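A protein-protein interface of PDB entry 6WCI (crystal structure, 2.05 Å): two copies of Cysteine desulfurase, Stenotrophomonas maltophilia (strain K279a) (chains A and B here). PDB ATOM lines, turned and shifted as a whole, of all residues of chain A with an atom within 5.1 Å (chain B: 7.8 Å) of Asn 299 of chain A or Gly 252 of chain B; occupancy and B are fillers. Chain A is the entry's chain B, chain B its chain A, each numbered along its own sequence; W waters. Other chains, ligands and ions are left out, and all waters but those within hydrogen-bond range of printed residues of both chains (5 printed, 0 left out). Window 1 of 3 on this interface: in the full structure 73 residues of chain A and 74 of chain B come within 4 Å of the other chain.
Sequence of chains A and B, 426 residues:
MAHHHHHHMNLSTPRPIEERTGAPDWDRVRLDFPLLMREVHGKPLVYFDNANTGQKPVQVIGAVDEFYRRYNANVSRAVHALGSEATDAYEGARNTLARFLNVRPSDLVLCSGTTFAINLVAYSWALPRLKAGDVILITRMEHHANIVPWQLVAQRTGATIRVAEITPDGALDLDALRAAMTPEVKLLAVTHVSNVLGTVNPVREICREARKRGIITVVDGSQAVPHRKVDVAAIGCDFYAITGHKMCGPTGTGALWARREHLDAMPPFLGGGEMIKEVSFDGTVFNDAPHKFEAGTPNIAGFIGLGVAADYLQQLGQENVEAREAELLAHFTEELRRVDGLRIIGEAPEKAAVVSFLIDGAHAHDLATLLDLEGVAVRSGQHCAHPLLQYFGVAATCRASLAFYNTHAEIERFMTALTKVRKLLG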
ATOM      1  N   TYR A  90     -27.927   2.140 -17.010  1.00  0.00           N
ATOM      2  CA  TYR A  90     -27.693   3.158 -15.994  1.00  0.00           C
ATOM      3  C   TYR A  90     -27.537   4.535 -16.624  1.00  0.00           C
ATOM      4  O   TYR A  90     -28.202   5.497 -16.218  1.00  0.00           O
ATOM      5  CB  TYR A  90     -26.463   2.780 -15.175  1.00  0.00           C
ATOM      6  CG  TYR A  90     -25.987   3.842 -14.213  1.00  0.00           C
ATOM      7  CD1 TYR A  90     -26.705   4.142 -13.056  1.00  0.00           C
ATOM      8  CD2 TYR A  90     -24.794   4.520 -14.440  1.00  0.00           C
ATOM      9  CE1 TYR A  90     -26.258   5.127 -12.167  1.00  0.00           C
ATOM     10  CE2 TYR A  90     -24.338   5.488 -13.562  1.00  0.00           C
ATOM     11  CZ  TYR A  90     -25.065   5.785 -12.427  1.00  0.00           C
ATOM     12  OH  TYR A  90     -24.588   6.753 -11.559  1.00  0.00           O
ATOM     13  N   THR A 251     -36.068   3.956  -3.693  1.00  0.00           N
ATOM     14  CA  THR A 251     -35.424   4.696  -2.628  1.00  0.00           C
ATOM     15  C   THR A 251     -33.920   4.816  -2.919  1.00  0.00           C
ATOM     16  O   THR A 251     -33.364   4.114  -3.769  1.00  0.00           O
ATOM     17  CB  THR A 251     -35.673   4.012  -1.282  1.00  0.00           C
ATOM     18  OG1 THR A 251     -35.143   2.688  -1.324  1.00  0.00           O
ATOM     19  CG2 THR A 251     -37.212   3.922  -0.964  1.00  0.00           C
ATOM     20  N   GLY A 252     -33.271   5.748  -2.223  1.00  0.00           N
ATOM     21  CA  GLY A 252     -31.853   5.995  -2.427  1.00  0.00           C
ATOM     22  C   GLY A 252     -31.491   6.574  -3.779  1.00  0.00           C
ATOM     23  O   GLY A 252     -30.379   6.345  -4.260  1.00  0.00           O
ATOM     24  N   THR A 253     -32.401   7.321  -4.407  1.00  0.00           N
ATOM     25  CA  THR A 253     -32.171   7.921  -5.714  1.00  0.00           C
ATOM     26  C   THR A 253     -32.600   9.386  -5.683  1.00  0.00           C
ATOM     27  O   THR A 253     -33.388   9.808  -4.836  1.00  0.00           O
ATOM     28  CB  THR A 253     -32.939   7.199  -6.833  1.00  0.00           C
ATOM     29  OG1 THR A 253     -34.340   7.269  -6.559  1.00  0.00           O
ATOM     30  CG2 THR A 253     -32.547   5.738  -6.932  1.00  0.00           C
ATOM     31  N   THR A 297     -19.225   3.017  -6.528  1.00  0.00           N
ATOM     32  CA  THR A 297     -20.272   2.301  -7.262  1.00  0.00           C
ATOM     33  C   THR A 297     -21.621   2.990  -7.052  1.00  0.00           C
ATOM     34  O   THR A 297     -22.010   3.257  -5.907  1.00  0.00           O
ATOM     35  CB  THR A 297     -20.349   0.830  -6.833  1.00  0.00           C
ATOM     36  OG1 THR A 297     -19.088   0.185  -7.057  1.00  0.00           O
ATOM     37  CG2 THR A 297     -21.407   0.082  -7.658  1.00  0.00           C
ATOM     38  N   PRO A 298     -22.351   3.309  -8.117  1.00  0.00           N
ATOM     39  CA  PRO A 298     -23.652   3.974  -7.953  1.00  0.00           C
ATOM     40  C   PRO A 298     -24.711   3.026  -7.408  1.00  0.00           C
ATOM     41  O   PRO A 298     -24.515   1.819  -7.251  1.00  0.00           O
ATOM     42  CB  PRO A 298     -24.001   4.428  -9.374  1.00  0.00           C
ATOM     43  CG  PRO A 298     -22.699   4.366 -10.144  1.00  0.00           C
ATOM     44  CD  PRO A 298     -21.962   3.207  -9.532  1.00  0.00           C
ATOM     45  N   ASN A 299     -25.875   3.601  -7.107  1.00  0.00           N
ATOM     46  CA  ASN A 299     -27.061   2.784  -6.849  1.00  0.00           C
ATOM     47  C   ASN A 299     -27.607   2.375  -8.211  1.00  0.00           C
ATOM     48  O   ASN A 299     -28.550   2.965  -8.739  1.00  0.00           O
ATOM     49  CB  ASN A 299     -28.092   3.559  -6.030  1.00  0.00           C
ATOM     50  CG  ASN A 299     -29.312   2.728  -5.686  1.00  0.00           C
ATOM     51  OD1 ASN A 299     -29.340   1.524  -5.934  1.00  0.00           O
ATOM     52  ND2 ASN A 299     -30.346   3.379  -5.132  1.00  0.00           N
ATOM     53  N   ILE A 300     -26.977   1.351  -8.797  1.00  0.00           N
ATOM     54  CA  ILE A 300     -27.285   0.972 -10.172  1.00  0.00           C
ATOM     55  C   ILE A 300     -28.745   0.568 -10.303  1.00  0.00           C
ATOM     56  O   ILE A 300     -29.444   0.993 -11.228  1.00  0.00           O
ATOM     57  CB  ILE A 300     -26.375  -0.177 -10.643  1.00  0.00           C
ATOM     58  CG1 ILE A 300     -24.898   0.203 -10.529  1.00  0.00           C
ATOM     59  CG2 ILE A 300     -26.697  -0.498 -12.061  1.00  0.00           C
ATOM     60  CD1 ILE A 300     -23.962  -0.986 -10.790  1.00  0.00           C
ATOM     61  N   ALA A 301     -29.211  -0.300  -9.406  1.00  0.00           N
ATOM     62  CA  ALA A 301     -30.575  -0.804  -9.513  1.00  0.00           C
ATOM     63  C   ALA A 301     -31.572   0.316  -9.285  1.00  0.00           C
ATOM     64  O   ALA A 301     -32.527   0.478 -10.053  1.00  0.00           O
ATOM     65  CB  ALA A 301     -30.798  -1.932  -8.511  1.00  0.00           C
ATOM     66  N   GLY A 302     -31.346   1.106  -8.238  1.00  0.00           N
ATOM     67  CA  GLY A 302     -32.240   2.213  -7.953  1.00  0.00           C
ATOM     68  C   GLY A 302     -32.362   3.181  -9.114  1.00  0.00           C
ATOM     69  O   GLY A 302     -33.462   3.619  -9.455  1.00  0.00           O
ATOM     70  N   PHE A 303     -31.237   3.526  -9.749  1.00  0.00           N
ATOM     71  CA  PHE A 303     -31.325   4.494 -10.839  1.00  0.00           C
ATOM     72  C   PHE A 303     -31.898   3.894 -12.118  1.00  0.00           C
ATOM     73  O   PHE A 303     -32.571   4.605 -12.875  1.00  0.00           O
ATOM     74  CB  PHE A 303     -29.964   5.150 -11.072  1.00  0.00           C
ATOM     75  CG  PHE A 303     -29.719   6.275 -10.124  1.00  0.00           C
ATOM     76  CD1 PHE A 303     -30.378   7.482 -10.299  1.00  0.00           C
ATOM     77  CD2 PHE A 303     -28.921   6.103  -9.005  1.00  0.00           C
ATOM     78  CE1 PHE A 303     -30.211   8.519  -9.402  1.00  0.00           C
ATOM     79  CE2 PHE A 303     -28.763   7.130  -8.107  1.00  0.00           C
ATOM     80  CZ  PHE A 303     -29.399   8.344  -8.313  1.00  0.00           C
ATOM     81  N   ILE A 304     -31.674   2.610 -12.380  1.00  0.00           N
ATOM     82  CA  ILE A 304     -32.391   1.971 -13.481  1.00  0.00           C
ATOM     83  C   ILE A 304     -33.899   2.066 -13.264  1.00  0.00           C
ATOM     84  O   ILE A 304     -34.657   2.377 -14.192  1.00  0.00           O
ATOM     85  CB  ILE A 304     -31.935   0.516 -13.642  1.00  0.00           C
ATOM     86  CG1 ILE A 304     -30.520   0.480 -14.217  1.00  0.00           C
ATOM     87  CG2 ILE A 304     -32.910  -0.275 -14.536  1.00  0.00           C
ATOM     88  CD1 ILE A 304     -30.012  -0.930 -14.340  1.00  0.00           C
ATOM     89  N   TYR B  68     -41.685  -3.035  -2.127  1.00  0.00           N
ATOM     90  CA  TYR B  68     -42.367  -2.149  -3.063  1.00  0.00           C
ATOM     91  C   TYR B  68     -43.813  -2.583  -3.309  1.00  0.00           C
ATOM     92  O   TYR B  68     -44.682  -1.733  -3.533  1.00  0.00           O
ATOM     93  CB  TYR B  68     -41.579  -2.081  -4.371  1.00  0.00           C
ATOM     94  CG  TYR B  68     -40.288  -1.273  -4.280  1.00  0.00           C
ATOM     95  CD1 TYR B  68     -40.272  -0.011  -3.707  1.00  0.00           C
ATOM     96  CD2 TYR B  68     -39.091  -1.784  -4.769  1.00  0.00           C
ATOM     97  CE1 TYR B  68     -39.099   0.731  -3.632  1.00  0.00           C
ATOM     98  CE2 TYR B  68     -37.902  -1.061  -4.685  1.00  0.00           C
ATOM     99  CZ  TYR B  68     -37.915   0.197  -4.119  1.00  0.00           C
ATOM    100  OH  TYR B  68     -36.757   0.922  -4.049  1.00  0.00           O
ATOM    101  N   LEU B 110     -25.323   3.506   8.612  1.00  0.00           N
ATOM    102  CA  LEU B 110     -25.714   2.927   7.335  1.00  0.00           C
ATOM    103  C   LEU B 110     -25.551   3.990   6.260  1.00  0.00           C
ATOM    104  O   LEU B 110     -25.970   5.130   6.455  1.00  0.00           O
ATOM    105  CB  LEU B 110     -27.164   2.432   7.391  1.00  0.00           C
ATOM    106  CG  LEU B 110     -27.510   1.368   8.438  1.00  0.00           C
ATOM    107  CD1 LEU B 110     -28.988   1.017   8.342  1.00  0.00           C
ATOM    108  CD2 LEU B 110     -26.623   0.105   8.233  1.00  0.00           C
ATOM    109  N   CYS B 111     -24.970   3.615   5.126  1.00  0.00           N
ATOM    110  CA  CYS B 111     -24.721   4.580   4.063  1.00  0.00           C
ATOM    111  C   CYS B 111     -24.707   3.857   2.719  1.00  0.00           C
ATOM    112  O   CYS B 111     -24.908   2.641   2.639  1.00  0.00           O
ATOM    113  CB  CYS B 111     -23.419   5.331   4.326  1.00  0.00           C
ATOM    114  SG  CYS B 111     -22.059   4.190   4.646  1.00  0.00           S
ATOM    115  N   SER B 112     -24.462   4.625   1.656  1.00  0.00           N
ATOM    116  CA  SER B 112     -24.585   4.166   0.278  1.00  0.00           C
ATOM    117  C   SER B 112     -23.428   3.284  -0.190  1.00  0.00           C
ATOM    118  O   SER B 112     -23.458   2.831  -1.344  1.00  0.00           O
ATOM    119  CB  SER B 112     -24.679   5.365  -0.658  1.00  0.00           C
ATOM    120  OG  SER B 112     -23.460   6.104  -0.624  1.00  0.00           O
ATOM    121  N   GLY B 113     -22.423   3.034   0.633  1.00  0.00           N
ATOM    122  CA  GLY B 113     -21.310   2.211   0.198  1.00  0.00           C
ATOM    123  C   GLY B 113     -20.057   2.495   0.996  1.00  0.00           C
ATOM    124  O   GLY B 113     -20.029   3.377   1.850  1.00  0.00           O
ATOM    125  N   THR B 243     -19.320  -2.594   2.031  1.00  0.00           N
ATOM    126  CA  THR B 243     -20.205  -2.210   0.952  1.00  0.00           C
ATOM    127  C   THR B 243     -21.118  -3.381   0.626  1.00  0.00           C
ATOM    128  O   THR B 243     -20.678  -4.539   0.563  1.00  0.00           O
ATOM    129  CB  THR B 243     -19.387  -1.707  -0.248  1.00  0.00           C
ATOM    130  OG1 THR B 243     -20.238  -0.960  -1.119  1.00  0.00           O
ATOM    131  CG2 THR B 243     -18.704  -2.856  -1.008  1.00  0.00           C
ATOM    132  N   GLY B 244     -22.406  -3.068   0.459  1.00  0.00           N
ATOM    133  CA  GLY B 244     -23.421  -4.111   0.475  1.00  0.00           C
ATOM    134  C   GLY B 244     -23.487  -4.929  -0.802  1.00  0.00           C
ATOM    135  O   GLY B 244     -23.799  -6.130  -0.765  1.00  0.00           O
ATOM    136  N   HIS B 245     -23.221  -4.299  -1.947  1.00  0.00           N
ATOM    137  CA  HIS B 245     -23.465  -4.959  -3.217  1.00  0.00           C
ATOM    138  C   HIS B 245     -22.458  -6.079  -3.484  1.00  0.00           C
ATOM    139  O   HIS B 245     -22.636  -6.868  -4.411  1.00  0.00           O
ATOM    140  CB  HIS B 245     -23.462  -3.947  -4.365  1.00  0.00           C
ATOM    141  CG  HIS B 245     -22.116  -3.354  -4.659  1.00  0.00           C
ATOM    142  ND1 HIS B 245     -21.338  -3.772  -5.721  1.00  0.00           N
ATOM    143  CD2 HIS B 245     -21.410  -2.378  -4.036  1.00  0.00           C
ATOM    144  CE1 HIS B 245     -20.204  -3.093  -5.728  1.00  0.00           C
ATOM    145  NE2 HIS B 245     -20.222  -2.244  -4.714  1.00  0.00           N
ATOM    146  N1  LLP B 246     -12.518  -0.863  -1.448  1.00  0.00           N
ATOM    147  C2  LLP B 246     -12.449  -2.098  -1.966  1.00  0.00           C
ATOM    148  C2' LLP B 246     -11.357  -3.003  -1.474  1.00  0.00           C
ATOM    149  C3  LLP B 246     -13.383  -2.547  -2.904  1.00  0.00           C
ATOM    150  O3  LLP B 246     -13.140  -3.739  -3.525  1.00  0.00           O
ATOM    151  C4  LLP B 246     -14.418  -1.701  -3.318  1.00  0.00           C
ATOM    152  C4' LLP B 246     -15.432  -2.128  -4.351  1.00  0.00           C
ATOM    153  C5  LLP B 246     -14.476  -0.418  -2.764  1.00  0.00           C
ATOM    154  C6  LLP B 246     -13.515  -0.063  -1.847  1.00  0.00           C
ATOM    155  C5' LLP B 246     -15.526   0.583  -3.177  1.00  0.00           C
ATOM    156  OP4 LLP B 246     -16.867   0.191  -2.762  1.00  0.00           O
ATOM    157  P   LLP B 246     -18.138   0.995  -3.396  1.00  0.00           P
ATOM    158  OP1 LLP B 246     -17.948   1.210  -4.847  1.00  0.00           O
ATOM    159  OP2 LLP B 246     -19.354   0.198  -3.067  1.00  0.00           O
ATOM    160  OP3 LLP B 246     -18.239   2.295  -2.648  1.00  0.00           O
ATOM    161  N   LLP B 246     -21.414  -6.160  -2.662  1.00  0.00           N
ATOM    162  CA  LLP B 246     -20.383  -7.189  -2.856  1.00  0.00           C
ATOM    163  CB  LLP B 246     -18.935  -6.690  -2.599  1.00  0.00           C
ATOM    164  CG  LLP B 246     -18.548  -5.720  -3.709  1.00  0.00           C
ATOM    165  CD  LLP B 246     -17.187  -5.078  -3.510  1.00  0.00           C
ATOM    166  CE  LLP B 246     -16.811  -4.118  -4.615  1.00  0.00           C
ATOM    167  NZ  LLP B 246     -15.458  -3.586  -4.434  1.00  0.00           N
ATOM    168  C   LLP B 246     -20.682  -8.334  -1.890  1.00  0.00           C
ATOM    169  O   LLP B 246     -20.066  -9.379  -1.966  1.00  0.00           O
ATOM    170  N   GLY B 249     -25.935  -8.169  -1.383  1.00  0.00           N
ATOM    171  CA  GLY B 249     -26.905  -7.147  -1.039  1.00  0.00           C
ATOM    172  C   GLY B 249     -27.246  -6.207  -2.180  1.00  0.00           C
ATOM    173  O   GLY B 249     -26.574  -6.174  -3.215  1.00  0.00           O
ATOM    174  N   PRO B 250     -28.311  -5.419  -2.008  1.00  0.00           N
ATOM    175  CA  PRO B 250     -28.689  -4.430  -3.027  1.00  0.00           C
ATOM    176  C   PRO B 250     -27.629  -3.351  -3.221  1.00  0.00           C
ATOM    177  O   PRO B 250     -26.815  -3.075  -2.343  1.00  0.00           O
ATOM    178  CB  PRO B 250     -29.975  -3.823  -2.458  1.00  0.00           C
ATOM    179  CG  PRO B 250     -30.532  -4.909  -1.591  1.00  0.00           C
ATOM    180  CD  PRO B 250     -29.319  -5.520  -0.942  1.00  0.00           C
ATOM    181  N   THR B 251     -27.660  -2.719  -4.390  1.00  0.00           N
ATOM    182  CA  THR B 251     -26.789  -1.574  -4.603  1.00  0.00           C
ATOM    183  C   THR B 251     -27.209  -0.410  -3.698  1.00  0.00           C
ATOM    184  O   THR B 251     -28.317  -0.377  -3.135  1.00  0.00           O
ATOM    185  CB  THR B 251     -26.811  -1.116  -6.066  1.00  0.00           C
ATOM    186  OG1 THR B 251     -28.175  -0.925  -6.494  1.00  0.00           O
ATOM    187  CG2 THR B 251     -26.072  -2.129  -6.985  1.00  0.00           C
ATOM    188  N   GLY B 252     -26.303   0.559  -3.570  1.00  0.00           N
ATOM    189  CA  GLY B 252     -26.570   1.737  -2.770  1.00  0.00           C
ATOM    190  C   GLY B 252     -26.651   1.464  -1.287  1.00  0.00           C
ATOM    191  O   GLY B 252     -27.324   2.202  -0.565  1.00  0.00           O
ATOM    192  N   THR B 253     -25.993   0.411  -0.811  1.00  0.00           N
ATOM    193  CA  THR B 253     -26.001   0.078   0.602  1.00  0.00           C
ATOM    194  C   THR B 253     -24.566  -0.120   1.070  1.00  0.00           C
ATOM    195  O   THR B 253     -23.652  -0.356   0.279  1.00  0.00           O
ATOM    196  CB  THR B 253     -26.837  -1.179   0.902  1.00  0.00           C
ATOM    197  OG1 THR B 253     -26.170  -2.340   0.388  1.00  0.00           O
ATOM    198  CG2 THR B 253     -28.200  -1.078   0.263  1.00  0.00           C
ATOM    199  N   GLY B 254     -24.386  -0.026   2.377  1.00  0.00           N
ATOM    200  CA  GLY B 254     -23.063  -0.071   2.959  1.00  0.00           C
ATOM    201  C   GLY B 254     -23.153   0.385   4.393  1.00  0.00           C
ATOM    202  O   GLY B 254     -24.232   0.710   4.897  1.00  0.00           O
ATOM    203  N   PRO B 298     -33.592   7.334   4.155  1.00  0.00           N
ATOM    204  CA  PRO B 298     -32.589   6.314   3.845  1.00  0.00           C
ATOM    205  C   PRO B 298     -32.962   5.523   2.603  1.00  0.00           C
ATOM    206  O   PRO B 298     -34.096   5.564   2.115  1.00  0.00           O
ATOM    207  CB  PRO B 298     -32.607   5.408   5.081  1.00  0.00           C
ATOM    208  CG  PRO B 298     -33.593   6.032   6.049  1.00  0.00           C
ATOM    209  CD  PRO B 298     -34.470   6.921   5.262  1.00  0.00           C
ATOM    210  N   ASN B 299     -31.988   4.741   2.110  1.00  0.00           N
ATOM    211  CA  ASN B 299     -32.295   3.776   1.055  1.00  0.00           C
ATOM    212  C   ASN B 299     -33.047   2.628   1.720  1.00  0.00           C
ATOM    213  O   ASN B 299     -32.489   1.576   2.033  1.00  0.00           O
ATOM    214  CB  ASN B 299     -31.038   3.289   0.337  1.00  0.00           C
ATOM    215  CG  ASN B 299     -31.351   2.255  -0.734  1.00  0.00           C
ATOM    216  OD1 ASN B 299     -32.514   2.039  -1.070  1.00  0.00           O
ATOM    217  ND2 ASN B 299     -30.317   1.609  -1.270  1.00  0.00           N
ATOM    218  N   ILE B 300     -34.348   2.843   1.944  1.00  0.00           N
ATOM    219  CA  ILE B 300     -35.103   1.908   2.779  1.00  0.00           C
ATOM    220  C   ILE B 300     -35.128   0.516   2.150  1.00  0.00           C
ATOM    221  O   ILE B 300     -34.858  -0.490   2.816  1.00  0.00           O
ATOM    222  CB  ILE B 300     -36.531   2.412   3.023  1.00  0.00           C
ATOM    223  CG1 ILE B 300     -36.552   3.793   3.702  1.00  0.00           C
ATOM    224  CG2 ILE B 300     -37.262   1.388   3.859  1.00  0.00           C
ATOM    225  CD1 ILE B 300     -37.968   4.423   3.725  1.00  0.00           C
ATOM    226  N   GLY B 302     -33.172  -0.835  -0.116  1.00  0.00           N
ATOM    227  CA  GLY B 302     -31.869  -1.482  -0.225  1.00  0.00           C
ATOM    228  C   GLY B 302     -31.403  -2.086   1.086  1.00  0.00           C
ATOM    229  O   GLY B 302     -30.910  -3.220   1.127  1.00  0.00           O
ATOM    230  N   PHE B 303     -31.607  -1.368   2.186  1.00  0.00           N
ATOM    231  CA  PHE B 303     -31.164  -1.889   3.472  1.00  0.00           C
ATOM    232  C   PHE B 303     -32.058  -2.998   3.994  1.00  0.00           C
ATOM    233  O   PHE B 303     -31.567  -3.894   4.686  1.00  0.00           O
ATOM    234  CB  PHE B 303     -31.044  -0.748   4.475  1.00  0.00           C
ATOM    235  CG  PHE B 303     -29.777   0.019   4.302  1.00  0.00           C
ATOM    236  CD1 PHE B 303     -28.588  -0.511   4.757  1.00  0.00           C
ATOM    237  CD2 PHE B 303     -29.760   1.212   3.606  1.00  0.00           C
ATOM    238  CE1 PHE B 303     -27.400   0.152   4.572  1.00  0.00           C
ATOM    239  CE2 PHE B 303     -28.568   1.880   3.415  1.00  0.00           C
ATOM    240  CZ  PHE B 303     -27.392   1.344   3.896  1.00  0.00           C
ATOM    241  N   LEU B 306     -30.337  -5.735   2.381  1.00  0.00           N
ATOM    242  CA  LEU B 306     -29.033  -6.047   2.957  1.00  0.00           C
ATOM    243  C   LEU B 306     -29.200  -6.804   4.264  1.00  0.00           C
ATOM    244  O   LEU B 306     -28.439  -7.733   4.553  1.00  0.00           O
ATOM    245  CB  LEU B 306     -28.211  -4.768   3.163  1.00  0.00           C
ATOM    246  CG  LEU B 306     -26.759  -4.942   3.629  1.00  0.00           C
ATOM    247  CD1 LEU B 306     -25.943  -5.806   2.643  1.00  0.00           C
ATOM    248  CD2 LEU B 306     -26.085  -3.599   3.817  1.00  0.00           C
HETATM  249  O   HOH W   1     -34.491   7.058  -0.441  1.00  0.00           O
HETATM  250  O   HOH W   2     -20.425   3.605  -3.556  1.00  0.00           O
HETATM  251  O   HOH W   3     -23.898   3.780  -3.976  1.00  0.00           O
HETATM  252  O   HOH W   4     -24.057   0.443  -5.067  1.00  0.00           O
HETATM  253  O   HOH W   5     -31.185  -0.215  -3.580  1.00  0.00           O
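The side-chain hydroxyl of Tyr 68 of chain B sits at hydrogen-bond distance from the backbone NH of Thr 251 of chain A, 3.1 Å away. The side-chain hydroxyl (OG1) of Thr 297 of chain A lies within hydrogen-bond range of OP1 of LLP 246 of chain B. OG1 of Thr 251 of chain B lies within hydrogen-bond range of OD1 of Asn 299 of chain A. The backbone NH of Ile 300 of chain A sits at hydrogen-bond distance from the side-chain hydroxyl of Thr 251 of chain B (3.5 Å). The side-chain hydroxyl (OG1) of Thr 251 of chain B is in hydrogen-bond range of the backbone NH (N) of Ala 301 of chain A (3.2 Å). The side-chain hydroxyl (OG1) of Thr 251 of chain A sits at hydrogen-bond distance from the side-chain amide oxygen (OD1) of Asn 299 of chain B, at 2.7 Å. N of Ile 300 of chain B sits at hydrogen-bond distance from OG1 of Thr 251 of chain A, at 3.4 Å.
A ring nitrogen (NE2) of His 245 of chain B sits at hydrogen-bond distance from OP2 of LLP 246 of chain B (3.1 Å). The side-chain amide nitrogen of Asn 299 of chain B sits at hydrogen-bond distance from the backbone carbonyl oxygen of Thr 251 of chain B (3.4 Å). O of Gly 252 of chain B lies within hydrogen-bond range of ND2 of Asn 299 of chain B. OD1 of Asn 299 of chain B sits at hydrogen-bond distance from N of Gly 302 of chain B. The backbone carbonyl oxygen of Gly 252 of chain A lies within hydrogen-bond range of the side-chain amide nitrogen of Asn 299 of chain A, at 3.1 Å. The backbone NH of Gly 302 of chain A lies within hydrogen-bond range of the side-chain amide oxygen of Asn 299 of chain A (3.1 Å).
Asn 299 of chain B touches Gly 252 of chain A (CA to N, 3.9 Å). NE2 of His 245 of chain B touches OG1 of Thr 297 of chain A (3.6 Å). Thr 251 of chain B touches Pro 298 of chain A. Gly 252 of chain B touches Asn 299 of chain A.
Asn 299 of chain A touches just these residues of chain B: Thr 251 and Gly 252. Gly 252 of chain B touches one residue of chain A. Of the printed residues of chain B, Thr 297 of chain A touches His 245 and LLP 246. Of the printed residues of chain B, Ile 300 of chain A touches Thr 251 (3.5 Å). Gly 254 of chain B touches none of the printed residues of chain A. The nearest residue of chain B that does not touch Asn 299 of chain A is Asn 299 of chain B (4.2 Å). The nearest residue of chain A that does not touch Gly 252 of chain B is Pro 298 of chain A (4.3 Å).
Of the 12 printed residues of chain A, 7 touch a printed residue of chain B. Printed residues of chain A that touch a printed residue of chain B: Thr 251, Gly 252, Thr 297, Pro 298, Asn 299, Ile 300 and Ala 301. Hydrophobic or aromatic side chains of chain A that line the printed part of chain B: Ala 301. Of the 21 printed residues of chain B, 7 touch a printed residue of chain A. Hydrophobic or aromatic side chains of chain B within 4 Å of the printed part of chain A: Tyr 68 and His 245. Among the printed residues, 11 pairs touch across the chains. Among the printed residues, no Asp or Glu carboxylate lies within 4 Å of a Lys or Arg side-chain nitrogen of the other chain.
Thr 251 of chain A touches Asn 299 of chain B, and with the chains exchanged Asn 299 of chain A touches Thr 251 of chain B. Thr 251 of chain A touches Ile 300 of chain B, and with the chains exchanged Ile 300 of chain A touches Thr 251 of chain B. Gly 252 of chain A touches Asn 299 of chain B, and with the chains exchanged Asn 299 of chain A touches Gly 252 of chain B. Pro 298 of chain A touches Thr 251 of chain B, but with the chains exchanged Thr 251 of chain A does not touch Pro 298 of chain B (4.1 Å).
Water W1 bridges N of Gly 252 of chain A and O of Pro 298 of chain B. Water W4 bridges the backbone carbonyl oxygen (O) of Pro 298 of chain A and the backbone NH (N) of Gly 252 of chain B. Water W2 lies within hydrogen-bond range of OP3 of LLP 246 of chain B (2.7 Å) and the backbone carbonyl oxygen (O) of Thr 297 of chain A (2.9 Å). Water W3 bridges O of Thr 297 of chain A (2.8 Å) and O of Ser 112 of chain B (2.8 Å). Water W5 lies within hydrogen-bond range of the backbone carbonyl oxygen (O) of Thr 251 of chain B (2.9 Å), the side-chain amide nitrogen (ND2) of Asn 299 of chain B (3.1 Å) and the side-chain amide oxygen (OD1) of Asn 299 of chain A (3.5 Å).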
